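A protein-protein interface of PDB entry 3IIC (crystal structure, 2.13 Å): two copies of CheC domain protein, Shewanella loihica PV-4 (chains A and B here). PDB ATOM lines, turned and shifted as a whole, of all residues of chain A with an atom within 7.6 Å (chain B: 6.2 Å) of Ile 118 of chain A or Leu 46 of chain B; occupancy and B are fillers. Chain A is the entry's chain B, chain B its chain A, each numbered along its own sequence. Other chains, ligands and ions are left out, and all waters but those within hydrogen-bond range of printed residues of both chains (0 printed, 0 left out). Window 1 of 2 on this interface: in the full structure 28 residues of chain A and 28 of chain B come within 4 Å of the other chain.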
ATOM      1  N   SER A  44      22.777  12.869  -8.342  1.00  0.00           N
ATOM      2  CA  SER A  44      22.409  11.766  -7.460  1.00  0.00           C
ATOM      3  C   SER A  44      23.592  11.252  -6.668  1.00  0.00           C
ATOM      4  O   SER A  44      24.693  11.172  -7.204  1.00  0.00           O
ATOM      5  CB  SER A  44      21.796  10.592  -8.250  1.00  0.00           C
ATOM      6  OG  SER A  44      20.552  10.978  -8.884  1.00  0.00           O
ATOM      7  N   GLY A  45      23.350  10.926  -5.392  1.00  0.00           N
ATOM      8  CA  GLY A  45      24.334  10.255  -4.536  1.00  0.00           C
ATOM      9  C   GLY A  45      23.885   8.809  -4.461  1.00  0.00           C
ATOM     10  O   GLY A  45      22.685   8.546  -4.214  1.00  0.00           O
ATOM     11  N   LEU A  46      24.825   7.885  -4.682  1.00  0.00           N
ATOM     12  CA  LEU A  46      24.570   6.438  -4.720  1.00  0.00           C
ATOM     13  C   LEU A  46      25.592   5.713  -3.815  1.00  0.00           C
ATOM     14  O   LEU A  46      26.770   6.039  -3.837  1.00  0.00           O
ATOM     15  CB  LEU A  46      24.669   5.898  -6.161  1.00  0.00           C
ATOM     16  CG  LEU A  46      23.699   6.400  -7.266  1.00  0.00           C
ATOM     17  CD1 LEU A  46      23.949   7.850  -7.679  1.00  0.00           C
ATOM     18  CD2 LEU A  46      23.817   5.552  -8.509  1.00  0.00           C
ATOM     19  N   ILE A  47      25.130   4.739  -3.033  1.00  0.00           N
ATOM     20  CA  ILE A  47      25.997   4.002  -2.118  1.00  0.00           C
ATOM     21  C   ILE A  47      25.494   2.563  -1.949  1.00  0.00           C
ATOM     22  O   ILE A  47      24.273   2.307  -1.830  1.00  0.00           O
ATOM     23  CB  ILE A  47      26.117   4.760  -0.754  1.00  0.00           C
ATOM     24  CG1 ILE A  47      27.310   4.243   0.067  1.00  0.00           C
ATOM     25  CG2 ILE A  47      24.788   4.754  -0.006  1.00  0.00           C
ATOM     26  CD1 ILE A  47      27.583   5.031   1.348  1.00  0.00           C
ATOM     27  N   GLY A  48      26.444   1.633  -1.988  1.00  0.00           N
ATOM     28  CA  GLY A  48      26.195   0.215  -1.812  1.00  0.00           C
ATOM     29  C   GLY A  48      26.344  -0.192  -0.357  1.00  0.00           C
ATOM     30  O   GLY A  48      27.184   0.366   0.377  1.00  0.00           O
ATOM     31  N   SER A  57      21.450  -1.248  -1.689  1.00  0.00           N
ATOM     32  CA  SER A  57      21.848   0.006  -2.323  1.00  0.00           C
ATOM     33  C   SER A  57      20.876   1.121  -2.006  1.00  0.00           C
ATOM     34  O   SER A  57      19.682   0.881  -1.845  1.00  0.00           O
ATOM     35  CB  SER A  57      21.955  -0.168  -3.838  1.00  0.00           C
ATOM     36  OG  SER A  57      20.774  -0.744  -4.354  1.00  0.00           O
ATOM     37  N   LEU A  58      21.422   2.332  -1.893  1.00  0.00           N
ATOM     38  CA  LEU A  58      20.667   3.556  -1.619  1.00  0.00           C
ATOM     39  C   LEU A  58      21.067   4.643  -2.625  1.00  0.00           C
ATOM     40  O   LEU A  58      22.243   4.777  -2.986  1.00  0.00           O
ATOM     41  CB  LEU A  58      20.893   4.039  -0.173  1.00  0.00           C
ATOM     42  CG  LEU A  58      20.350   5.420   0.321  1.00  0.00           C
ATOM     43  CD1 LEU A  58      20.026   5.413   1.779  1.00  0.00           C
ATOM     44  CD2 LEU A  58      21.283   6.599   0.050  1.00  0.00           C
ATOM     45  N   SER A  59      20.076   5.393  -3.086  1.00  0.00           N
ATOM     46  CA  SER A  59      20.291   6.512  -3.969  1.00  0.00           C
ATOM     47  C   SER A  59      19.457   7.696  -3.481  1.00  0.00           C
ATOM     48  O   SER A  59      18.324   7.501  -3.019  1.00  0.00           O
ATOM     49  CB  SER A  59      19.942   6.165  -5.414  1.00  0.00           C
ATOM     50  OG  SER A  59      18.571   5.829  -5.569  1.00  0.00           O
ATOM     51  N   ILE A  60      20.054   8.897  -3.546  1.00  0.00           N
ATOM     52  CA  ILE A  60      19.381  10.172  -3.214  1.00  0.00           C
ATOM     53  C   ILE A  60      19.572  11.002  -4.462  1.00  0.00           C
ATOM     54  O   ILE A  60      20.704  11.317  -4.806  1.00  0.00           O
ATOM     55  CB  ILE A  60      19.936  10.908  -1.929  1.00  0.00           C
ATOM     56  CG1 ILE A  60      19.980   9.961  -0.721  1.00  0.00           C
ATOM     57  CG2 ILE A  60      19.011  12.037  -1.548  1.00  0.00           C
ATOM     58  CD1 ILE A  60      20.484  10.599   0.591  1.00  0.00           C
ATOM     59  N   THR A  87      28.809  18.412  -6.357  1.00  0.00           N
ATOM     60  CA  THR A  87      28.944  16.953  -6.342  1.00  0.00           C
ATOM     61  C   THR A  87      29.556  16.439  -5.013  1.00  0.00           C
ATOM     62  O   THR A  87      29.155  15.355  -4.533  1.00  0.00           O
ATOM     63  CB  THR A  87      29.701  16.374  -7.556  1.00  0.00           C
ATOM     64  OG1 THR A  87      31.064  16.768  -7.492  1.00  0.00           O
ATOM     65  CG2 THR A  87      29.054  16.819  -8.876  1.00  0.00           C
ATOM     66  N   VAL A  90      26.772  16.546  -2.418  1.00  0.00           N
ATOM     67  CA  VAL A  90      25.924  15.365  -2.601  1.00  0.00           C
ATOM     68  C   VAL A  90      26.606  14.117  -2.019  1.00  0.00           C
ATOM     69  O   VAL A  90      25.953  13.347  -1.346  1.00  0.00           O
ATOM     70  CB  VAL A  90      25.420  15.184  -4.071  1.00  0.00           C
ATOM     71  CG1 VAL A  90      24.528  13.909  -4.247  1.00  0.00           C
ATOM     72  CG2 VAL A  90      24.616  16.455  -4.539  1.00  0.00           C
ATOM     73  N   GLY A  91      27.918  13.956  -2.215  1.00  0.00           N
ATOM     74  CA  GLY A  91      28.654  12.827  -1.640  1.00  0.00           C
ATOM     75  C   GLY A  91      28.568  12.850  -0.103  1.00  0.00           C
ATOM     76  O   GLY A  91      28.195  11.848   0.515  1.00  0.00           O
ATOM     77  N   THR A  94      25.070  12.041   1.137  1.00  0.00           N
ATOM     78  CA  THR A  94      24.833  10.583   0.988  1.00  0.00           C
ATOM     79  C   THR A  94      25.455   9.823   2.152  1.00  0.00           C
ATOM     80  O   THR A  94      24.819   8.912   2.700  1.00  0.00           O
ATOM     81  CB  THR A  94      25.354  10.036  -0.345  1.00  0.00           C
ATOM     82  OG1 THR A  94      24.729  10.775  -1.391  1.00  0.00           O
ATOM     83  CG2 THR A  94      25.025   8.527  -0.544  1.00  0.00           C
ATOM     84  N   ASN A  95      26.687  10.208   2.512  1.00  0.00           N
ATOM     85  CA  ASN A  95      27.354   9.640   3.681  1.00  0.00           C
ATOM     86  C   ASN A  95      26.627   9.904   4.990  1.00  0.00           C
ATOM     87  O   ASN A  95      26.509   8.988   5.779  1.00  0.00           O
ATOM     88  CB  ASN A  95      28.826  10.079   3.797  1.00  0.00           C
ATOM     89  CG  ASN A  95      29.759   9.232   2.977  1.00  0.00           C
ATOM     90  OD1 ASN A  95      29.401   8.169   2.481  1.00  0.00           O
ATOM     91  ND2 ASN A  95      30.992   9.669   2.888  1.00  0.00           N
ATOM     92  N   ALA A 115      29.748   1.068   1.338  1.00  0.00           N
ATOM     93  CA  ALA A 115      30.832   1.246   0.401  1.00  0.00           C
ATOM     94  C   ALA A 115      31.093   2.742   0.248  1.00  0.00           C
ATOM     95  O   ALA A 115      30.608   3.535   1.040  1.00  0.00           O
ATOM     96  CB  ALA A 115      30.483   0.602  -0.911  1.00  0.00           C
ATOM     97  N   THR A 116      31.945   3.092  -0.717  1.00  0.00           N
ATOM     98  CA  THR A 116      32.261   4.477  -1.140  1.00  0.00           C
ATOM     99  C   THR A 116      31.052   5.059  -1.863  1.00  0.00           C
ATOM    100  O   THR A 116      30.506   4.384  -2.732  1.00  0.00           O
ATOM    101  CB  THR A 116      33.433   4.448  -2.220  1.00  0.00           C
ATOM    102  OG1 THR A 116      34.680   4.138  -1.593  1.00  0.00           O
ATOM    103  CG2 THR A 116      33.581   5.773  -3.058  1.00  0.00           C
ATOM    104  N   PRO A 117      30.659   6.307  -1.568  1.00  0.00           N
ATOM    105  CA  PRO A 117      29.577   6.892  -2.379  1.00  0.00           C
ATOM    106  C   PRO A 117      30.029   7.323  -3.804  1.00  0.00           C
ATOM    107  O   PRO A 117      31.209   7.677  -4.024  1.00  0.00           O
ATOM    108  CB  PRO A 117      29.122   8.101  -1.556  1.00  0.00           C
ATOM    109  CG  PRO A 117      30.280   8.445  -0.728  1.00  0.00           C
ATOM    110  CD  PRO A 117      31.002   7.170  -0.425  1.00  0.00           C
ATOM    111  N   ILE A 118      29.099   7.210  -4.756  1.00  0.00           N
ATOM    112  CA  ILE A 118      29.291   7.654  -6.126  1.00  0.00           C
ATOM    113  C   ILE A 118      28.300   8.791  -6.403  1.00  0.00           C
ATOM    114  O   ILE A 118      27.125   8.676  -6.051  1.00  0.00           O
ATOM    115  CB  ILE A 118      29.056   6.525  -7.156  1.00  0.00           C
ATOM    116  CG1 ILE A 118      30.093   5.405  -6.956  1.00  0.00           C
ATOM    117  CG2 ILE A 118      29.183   7.070  -8.561  1.00  0.00           C
ATOM    118  CD1 ILE A 118      29.912   4.239  -7.896  1.00  0.00           C
ATOM    119  N   VAL A 119      28.774   9.874  -7.023  1.00  0.00           N
ATOM    120  CA  VAL A 119      27.908  10.964  -7.438  1.00  0.00           C
ATOM    121  C   VAL A 119      27.855  10.964  -8.968  1.00  0.00           C
ATOM    122  O   VAL A 119      28.890  10.995  -9.639  1.00  0.00           O
ATOM    123  CB  VAL A 119      28.311  12.368  -6.887  1.00  0.00           C
ATOM    124  CG1 VAL A 119      27.287  13.508  -7.411  1.00  0.00           C
ATOM    125  CG2 VAL A 119      28.351  12.342  -5.362  1.00  0.00           C
ATOM    126  N   VAL A 120      26.625  10.959  -9.480  1.00  0.00           N
ATOM    127  CA  VAL A 120      26.306  11.029 -10.886  1.00  0.00           C
ATOM    128  C   VAL A 120      25.743  12.431 -11.165  1.00  0.00           C
ATOM    129  O   VAL A 120      24.889  12.881 -10.410  1.00  0.00           O
ATOM    130  CB  VAL A 120      25.206  10.005 -11.257  1.00  0.00           C
ATOM    131  CG1 VAL A 120      24.896  10.059 -12.780  1.00  0.00           C
ATOM    132  CG2 VAL A 120      25.641   8.624 -10.840  1.00  0.00           C
ATOM    133  N   SER A 121      26.259  13.105 -12.199  1.00  0.00           N
ATOM    134  CA  SER A 121      25.806  14.431 -12.620  1.00  0.00           C
ATOM    135  C   SER A 121      25.359  14.302 -14.043  1.00  0.00           C
ATOM    136  O   SER A 121      26.134  13.870 -14.891  1.00  0.00           O
ATOM    137  CB  SER A 121      26.931  15.471 -12.538  1.00  0.00           C
ATOM    138  OG  SER A 121      27.395  15.607 -11.215  1.00  0.00           O
ATOM    139  N   ALA A 128      17.966   3.200 -11.579  1.00  0.00           N
ATOM    140  CA  ALA A 128      17.335   1.884 -11.462  1.00  0.00           C
ATOM    141  C   ALA A 128      18.239   1.019 -10.587  1.00  0.00           C
ATOM    142  O   ALA A 128      19.422   0.954 -10.848  1.00  0.00           O
ATOM    143  CB  ALA A 128      17.152   1.259 -12.819  1.00  0.00           C
ATOM    144  N   LYS A 130      19.163  -2.521  -9.759  1.00  0.00           N
ATOM    145  CA  LYS A 130      18.987  -3.808 -10.458  1.00  0.00           C
ATOM    146  C   LYS A 130      19.174  -4.971  -9.492  1.00  0.00           C
ATOM    147  O   LYS A 130      20.283  -5.405  -9.241  1.00  0.00           O
ATOM    148  CB  LYS A 130      19.925  -3.910 -11.660  1.00  0.00           C
ATOM    149  CG  LYS A 130      19.668  -2.860 -12.737  1.00  0.00           C
ATOM    150  CD  LYS A 130      18.401  -3.132 -13.536  1.00  0.00           C
ATOM    151  CE  LYS A 130      18.092  -2.019 -14.465  1.00  0.00           C
ATOM    152  NZ  LYS A 130      17.040  -2.438 -15.391  1.00  0.00           N
ATOM    153  N   SER B  44      25.252   3.823 -17.381  1.00  0.00           N
ATOM    154  CA  SER B  44      26.339   3.312 -16.529  1.00  0.00           C
ATOM    155  C   SER B  44      25.850   2.302 -15.485  1.00  0.00           C
ATOM    156  O   SER B  44      24.761   2.451 -14.927  1.00  0.00           O
ATOM    157  CB  SER B  44      27.034   4.458 -15.782  1.00  0.00           C
ATOM    158  OG  SER B  44      27.540   5.442 -16.653  1.00  0.00           O
ATOM    159  N   GLY B  45      26.659   1.268 -15.241  1.00  0.00           N
ATOM    160  CA  GLY B  45      26.412   0.331 -14.157  1.00  0.00           C
ATOM    161  C   GLY B  45      27.344   0.750 -13.020  1.00  0.00           C
ATOM    162  O   GLY B  45      28.535   0.987 -13.254  1.00  0.00           O
ATOM    163  N   LEU B  46      26.816   0.799 -11.795  1.00  0.00           N
ATOM    164  CA  LEU B  46      27.571   1.212 -10.579  1.00  0.00           C
ATOM    165  C   LEU B  46      27.391   0.214  -9.431  1.00  0.00           C
ATOM    166  O   LEU B  46      26.276  -0.224  -9.162  1.00  0.00           O
ATOM    167  CB  LEU B  46      27.152   2.626 -10.158  1.00  0.00           C
ATOM    168  CG  LEU B  46      27.354   3.665 -11.293  1.00  0.00           C
ATOM    169  CD1 LEU B  46      26.112   3.870 -12.149  1.00  0.00           C
ATOM    170  CD2 LEU B  46      27.730   5.000 -10.741  1.00  0.00           C
ATOM    171  N   ILE B  47      28.491  -0.160  -8.754  1.00  0.00           N
ATOM    172  CA  ILE B  47      28.433  -1.156  -7.701  1.00  0.00           C
ATOM    173  C   ILE B  47      29.493  -0.879  -6.605  1.00  0.00           C
ATOM    174  O   ILE B  47      30.682  -0.549  -6.903  1.00  0.00           O
ATOM    175  CB  ILE B  47      28.616  -2.576  -8.310  1.00  0.00           C
ATOM    176  CG1 ILE B  47      28.111  -3.657  -7.350  1.00  0.00           C
ATOM    177  CG2 ILE B  47      30.136  -2.849  -8.733  1.00  0.00           C
ATOM    178  CD1 ILE B  47      28.109  -5.090  -7.984  1.00  0.00           C
ATOM    179  N   GLY B  48      29.034  -0.986  -5.359  1.00  0.00           N
ATOM    180  CA  GLY B  48      29.866  -0.796  -4.205  1.00  0.00           C
ATOM    181  C   GLY B  48      30.495  -2.110  -3.752  1.00  0.00           C
ATOM    182  O   GLY B  48      29.964  -3.207  -4.006  1.00  0.00           O
ATOM    183  N   SER B  57      34.456   1.073  -4.872  1.00  0.00           N
ATOM    184  CA  SER B  57      33.393   1.252  -5.842  1.00  0.00           C
ATOM    185  C   SER B  57      33.861   1.071  -7.270  1.00  0.00           C
ATOM    186  O   SER B  57      35.017   1.337  -7.599  1.00  0.00           O
ATOM    187  CB  SER B  57      32.740   2.640  -5.651  1.00  0.00           C
ATOM    188  OG  SER B  57      33.715   3.684  -5.630  1.00  0.00           O
ATOM    189  N   LEU B  58      32.959   0.552  -8.094  1.00  0.00           N
ATOM    190  CA  LEU B  58      33.213   0.335  -9.497  1.00  0.00           C
ATOM    191  C   LEU B  58      32.073   0.923 -10.366  1.00  0.00           C
ATOM    192  O   LEU B  58      30.924   0.836  -9.988  1.00  0.00           O
ATOM    193  CB  LEU B  58      33.420  -1.153  -9.762  1.00  0.00           C
ATOM    194  CG  LEU B  58      33.600  -1.620 -11.209  1.00  0.00           C
ATOM    195  CD1 LEU B  58      34.571  -2.786 -11.264  1.00  0.00           C
ATOM    196  CD2 LEU B  58      32.275  -2.015 -11.818  1.00  0.00           C
ATOM    197  N   SER B  59      32.431   1.553 -11.485  1.00  0.00           N
ATOM    198  CA  SER B  59      31.436   2.005 -12.468  1.00  0.00           C
ATOM    199  C   SER B  59      31.915   1.647 -13.868  1.00  0.00           C
ATOM    200  O   SER B  59      33.110   1.625 -14.125  1.00  0.00           O
ATOM    201  CB  SER B  59      31.105   3.498 -12.340  1.00  0.00           C
ATOM    202  OG  SER B  59      32.215   4.328 -12.566  1.00  0.00           O
ATOM    203  N   ILE B  60      30.979   1.273 -14.724  1.00  0.00           N
ATOM    204  CA  ILE B  60      31.237   0.961 -16.133  1.00  0.00           C
ATOM    205  C   ILE B  60      30.194   1.803 -16.905  1.00  0.00           C
ATOM    206  O   ILE B  60      28.999   1.584 -16.742  1.00  0.00           O
ATOM    207  CB  ILE B  60      31.049  -0.542 -16.504  1.00  0.00           C
ATOM    208  CG1 ILE B  60      31.893  -1.494 -15.605  1.00  0.00           C
ATOM    209  CG2 ILE B  60      31.385  -0.717 -17.969  1.00  0.00           C
ATOM    210  CD1 ILE B  60      31.607  -3.007 -15.816  1.00  0.00           C
ATOM    211  N   VAL B  90      23.208  -3.867 -18.755  1.00  0.00           N
ATOM    212  CA  VAL B  90      24.268  -3.110 -18.114  1.00  0.00           C
ATOM    213  C   VAL B  90      24.436  -3.579 -16.658  1.00  0.00           C
ATOM    214  O   VAL B  90      25.570  -3.763 -16.232  1.00  0.00           O
ATOM    215  CB  VAL B  90      24.050  -1.564 -18.283  1.00  0.00           C
ATOM    216  CG1 VAL B  90      25.035  -0.752 -17.435  1.00  0.00           C
ATOM    217  CG2 VAL B  90      24.159  -1.180 -19.785  1.00  0.00           C
ATOM    218  N   THR B  94      27.716  -5.446 -15.266  1.00  0.00           N
ATOM    219  CA  THR B  94      28.331  -4.906 -14.039  1.00  0.00           C
ATOM    220  C   THR B  94      28.582  -5.967 -12.952  1.00  0.00           C
ATOM    221  O   THR B  94      29.657  -5.983 -12.395  1.00  0.00           O
ATOM    222  CB  THR B  94      27.532  -3.696 -13.465  1.00  0.00           C
ATOM    223  OG1 THR B  94      27.423  -2.702 -14.497  1.00  0.00           O
ATOM    224  CG2 THR B  94      28.245  -3.090 -12.241  1.00  0.00           C
ATOM    225  N   THR B 116      24.332  -4.377  -4.287  1.00  0.00           N
ATOM    226  CA  THR B 116      23.448  -4.563  -5.454  1.00  0.00           C
ATOM    227  C   THR B 116      23.844  -3.478  -6.478  1.00  0.00           C
ATOM    228  O   THR B 116      24.211  -2.365  -6.108  1.00  0.00           O
ATOM    229  CB  THR B 116      21.944  -4.488  -5.125  1.00  0.00           C
ATOM    230  OG1 THR B 116      21.707  -3.379  -4.269  1.00  0.00           O
ATOM    231  CG2 THR B 116      21.455  -5.728  -4.437  1.00  0.00           C
ATOM    232  N   PRO B 117      23.802  -3.803  -7.764  1.00  0.00           N
ATOM    233  CA  PRO B 117      24.200  -2.826  -8.773  1.00  0.00           C
ATOM    234  C   PRO B 117      23.110  -1.800  -9.077  1.00  0.00           C
ATOM    235  O   PRO B 117      21.921  -2.123  -8.964  1.00  0.00           O
ATOM    236  CB  PRO B 117      24.422  -3.682 -10.011  1.00  0.00           C
ATOM    237  CG  PRO B 117      23.592  -4.845  -9.821  1.00  0.00           C
ATOM    238  CD  PRO B 117      23.490  -5.111  -8.368  1.00  0.00           C
ATOM    239  N   ILE B 118      23.520  -0.585  -9.433  1.00  0.00           N
ATOM    240  CA  ILE B 118      22.586   0.473  -9.831  1.00  0.00           C
ATOM    241  C   ILE B 118      22.957   0.797 -11.280  1.00  0.00           C
ATOM    242  O   ILE B 118      24.154   0.789 -11.649  1.00  0.00           O
ATOM    243  CB  ILE B 118      22.691   1.728  -8.954  1.00  0.00           C
ATOM    244  CG1 ILE B 118      22.352   1.414  -7.494  1.00  0.00           C
ATOM    245  CG2 ILE B 118      21.794   2.878  -9.496  1.00  0.00           C
ATOM    246  CD1 ILE B 118      22.497   2.625  -6.527  1.00  0.00           C
ATOM    247  N   VAL B 119      21.939   1.016 -12.096  1.00  0.00           N
ATOM    248  CA  VAL B 119      22.120   1.485 -13.455  1.00  0.00           C
ATOM    249  C   VAL B 119      21.553   2.902 -13.596  1.00  0.00           C
ATOM    250  O   VAL B 119      20.435   3.151 -13.201  1.00  0.00           O
ATOM    251  CB  VAL B 119      21.560   0.533 -14.511  1.00  0.00           C
ATOM    252  CG1 VAL B 119      21.816   1.120 -15.907  1.00  0.00           C
ATOM    253  CG2 VAL B 119      22.221  -0.835 -14.369  1.00  0.00           C
ATOM    254  N   VAL B 120      22.365   3.803 -14.145  1.00  0.00           N
ATOM    255  CA  VAL B 120      22.026   5.200 -14.397  1.00  0.00           C
ATOM    256  C   VAL B 120      21.870   5.371 -15.878  1.00  0.00           C
ATOM    257  O   VAL B 120      22.721   4.935 -16.637  1.00  0.00           O
ATOM    258  CB  VAL B 120      23.166   6.176 -13.889  1.00  0.00           C
ATOM    259  CG1 VAL B 120      22.989   7.617 -14.427  1.00  0.00           C
ATOM    260  CG2 VAL B 120      23.159   6.209 -12.377  1.00  0.00           C
ATOM    261  N   HIS B 125      26.051  11.969 -18.949  1.00  0.00           N
ATOM    262  CA  HIS B 125      26.248  12.094 -17.500  1.00  0.00           C
ATOM    263  C   HIS B 125      27.706  11.787 -17.184  1.00  0.00           C
ATOM    264  O   HIS B 125      28.399  11.153 -17.999  1.00  0.00           O
ATOM    265  CB  HIS B 125      25.275  11.220 -16.671  1.00  0.00           C
ATOM    266  CG  HIS B 125      25.443   9.744 -16.855  1.00  0.00           C
ATOM    267  ND1 HIS B 125      24.664   9.007 -17.722  1.00  0.00           N
ATOM    268  CD2 HIS B 125      26.308   8.870 -16.281  1.00  0.00           C
ATOM    269  CE1 HIS B 125      25.041   7.743 -17.665  1.00  0.00           C
ATOM    270  NE2 HIS B 125      26.033   7.631 -16.796  1.00  0.00           N
ATOM    271  N   ILE B 127      30.482  10.816 -13.746  1.00  0.00           N
ATOM    272  CA  ILE B 127      30.577   9.998 -12.530  1.00  0.00           C
ATOM    273  C   ILE B 127      31.771  10.404 -11.673  1.00  0.00           C
ATOM    274  O   ILE B 127      32.878  10.499 -12.193  1.00  0.00           O
ATOM    275  CB  ILE B 127      30.713   8.492 -12.912  1.00  0.00           C
ATOM    276  CG1 ILE B 127      29.455   8.048 -13.687  1.00  0.00           C
ATOM    277  CG2 ILE B 127      30.957   7.593 -11.660  1.00  0.00           C
ATOM    278  CD1 ILE B 127      29.439   6.609 -14.082  1.00  0.00           C
ATOM    279  N   ALA B 128      31.506  10.658 -10.386  1.00  0.00           N
ATOM    280  CA  ALA B 128      32.512  11.004  -9.386  1.00  0.00           C
ATOM    281  C   ALA B 128      32.436   9.975  -8.264  1.00  0.00           C
ATOM    282  O   ALA B 128      31.382   9.808  -7.660  1.00  0.00           O
ATOM    283  CB  ALA B 128      32.279  12.397  -8.830  1.00  0.00           C
ATOM    284  N   HIS B 129      33.529   9.248  -8.024  1.00  0.00           N
ATOM    285  CA  HIS B 129      33.618   8.309  -6.890  1.00  0.00           C
ATOM    286  C   HIS B 129      34.206   9.155  -5.794  1.00  0.00           C
ATOM    287  O   HIS B 129      35.325   9.600  -5.922  1.00  0.00           O
ATOM    288  CB  HIS B 129      34.544   7.154  -7.211  1.00  0.00           C
ATOM    289  CG  HIS B 129      33.991   6.193  -8.196  1.00  0.00           C
ATOM    290  ND1 HIS B 129      34.002   4.834  -7.979  1.00  0.00           N
ATOM    291  CD2 HIS B 129      33.382   6.385  -9.393  1.00  0.00           C
ATOM    292  CE1 HIS B 129      33.473   4.226  -9.035  1.00  0.00           C
ATOM    293  NE2 HIS B 129      33.088   5.146  -9.907  1.00  0.00           N
ATOM    294  N   LYS B 130      33.457   9.392  -4.724  1.00  0.00           N
ATOM    295  CA  LYS B 130      33.892  10.270  -3.639  1.00  0.00           C
ATOM    296  C   LYS B 130      34.648   9.493  -2.533  1.00  0.00           C
ATOM    297  O   LYS B 130      34.050   9.008  -1.567  1.00  0.00           O
ATOM    298  CB  LYS B 130      32.688  11.065  -3.095  1.00  0.00           C
ATOM    299  CG  LYS B 130      32.028  11.948  -4.146  1.00  0.00           C
ATOM    300  CD  LYS B 130      32.974  13.023  -4.730  1.00  0.00           C
ATOM    301  CE  LYS B 130      32.223  14.023  -5.600  1.00  0.00           C
ATOM    302  NZ  LYS B 130      33.076  15.064  -6.267  1.00  0.00           N
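Of the 21 printed residues of chain B, 13 touch a printed residue of chain A. Hydrophobic or aromatic side chains of chain B within 4 Å of the printed part of chain A: Leu 46, Pro 117, Ile 118, Val 119, Val 120, His 125, Ile 127, Ala 128 and His 129. Printed residues of chain A that touch a printed residue of chain B: Leu 46, Ser 57, Thr 87, Ala 115, Thr 116, Pro 117, Ile 118, Val 119, Val 120, Ser 121, Ala 128 and Lys 130. Hydrophobic or aromatic side chains of chain A that line the printed part of chain B: Leu 46, Ala 115, Pro 117, Ile 118, Val 119, Val 120 and Ala 128.
Lys 130 of chain B touches Thr 116 of chain A (O to CG2, 3.6 Å). Pro 117 of chain A touches His 129 of chain B. Ile 118 of chain A touches Ser 57 of chain B (CD1 to CB, 3.9 Å). Ile 118 of chain A touches Ile 127 of chain B. CD1 of Ile 118 of chain A touches CE1 of His 129 of chain B, at 3.7 Å. Val 120 of chain B touches Val 120 of chain A. Val 120 of chain A touches His 125 of chain B (CG1 to CD2, 3.96 Å). His 125 of chain B touches Ser 121 of chain A. Ile 118 of chain B touches Ala 128 of chain A.
Ile 118 of chain A touches Ala 128 of chain B, and with the chains exchanged Ala 128 of chain A touches Ile 118 of chain B. Val 119 of chain A touches Ala 128 of chain B, and with the chains exchanged Ala 128 of chain A touches Val 119 of chain B. Val 119 of chain A touches Lys 130 of chain B, and with the chains exchanged Lys 130 of chain A touches Val 119 of chain B. Val 120 of chain A touches its own counterpart, Val 120 of chain B.
The backbone NH (N) of Leu 46 of chain B lies within hydrogen-bond range of the backbone carbonyl oxygen (O) of Ile 118 of chain B (2.7 Å). The backbone carbonyl oxygen (O) of Ser 44 of chain B sits at hydrogen-bond distance from the backbone NH (N) of Val 120 of chain B, at 2.9 Å. OG of Ser 57 of chain B lies within hydrogen-bond range of ND1 of His 129 of chain B (2.6 Å). The backbone NH (N) of Ser 44 of chain A sits at hydrogen-bond distance from the backbone carbonyl oxygen (O) of Val 120 of chain A (3.0 Å).
The backbone NH (N) of Val 119 of chain A lies within hydrogen-bond range of the backbone carbonyl oxygen (O) of Ala 128 of chain B, at 2.7 Å. The side-chain hydroxyl (OG1) of Thr 87 of chain A lies within hydrogen-bond range of the side-chain amino group (NZ) of Lys 130 of chain B, 2.9 Å away. OG of Ser 57 of chain A is in hydrogen-bond range of OG1 of Thr 116 of chain B (2.8 Å). The backbone carbonyl oxygen (O) of Pro 117 of chain B sits at hydrogen-bond distance from the backbone NH (N) of Lys 130 of chain A. N of Val 119 of chain B is in hydrogen-bond range of O of Ala 128 of chain A. O of Pro 117 of chain A lies within hydrogen-bond range of N of Lys 130 of chain B (2.9 Å).
Printed residues of chain B within 4 Å of Leu 46 of chain A: Ile 118 (3.5 Å) and Val 120 (3.98 Å). Ile 118 of chain A touches just these residues of chain B: Leu 46, Ser 57, Ile 127, Ala 128 and His 129. Printed residues of chain B within 4 Å of Ser 121 of chain A: His 125 (3.2 Å). Printed residues of chain B within 4 Å of Lys 130 of chain A: Pro 117 (2.9 Å) and Val 119 (3.6 Å). No residue of chain A comes within 4 Å of Gly 45 of chain B. Of chain A, only Ile 118 comes within 4 Å of Leu 46 of chain B. Printed residues of chain A within 4 Å of His 129 of chain B: Pro 117 (3.8 Å) and Ile 118 (3.7 Å). Of the printed residues of chain A, Lys 130 of chain B touches Thr 87, Thr 116, Pro 117 and Val 119. The nearest residue of chain B that does not touch Ile 118 of chain A is Leu 58 of chain B (4.1 Å).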
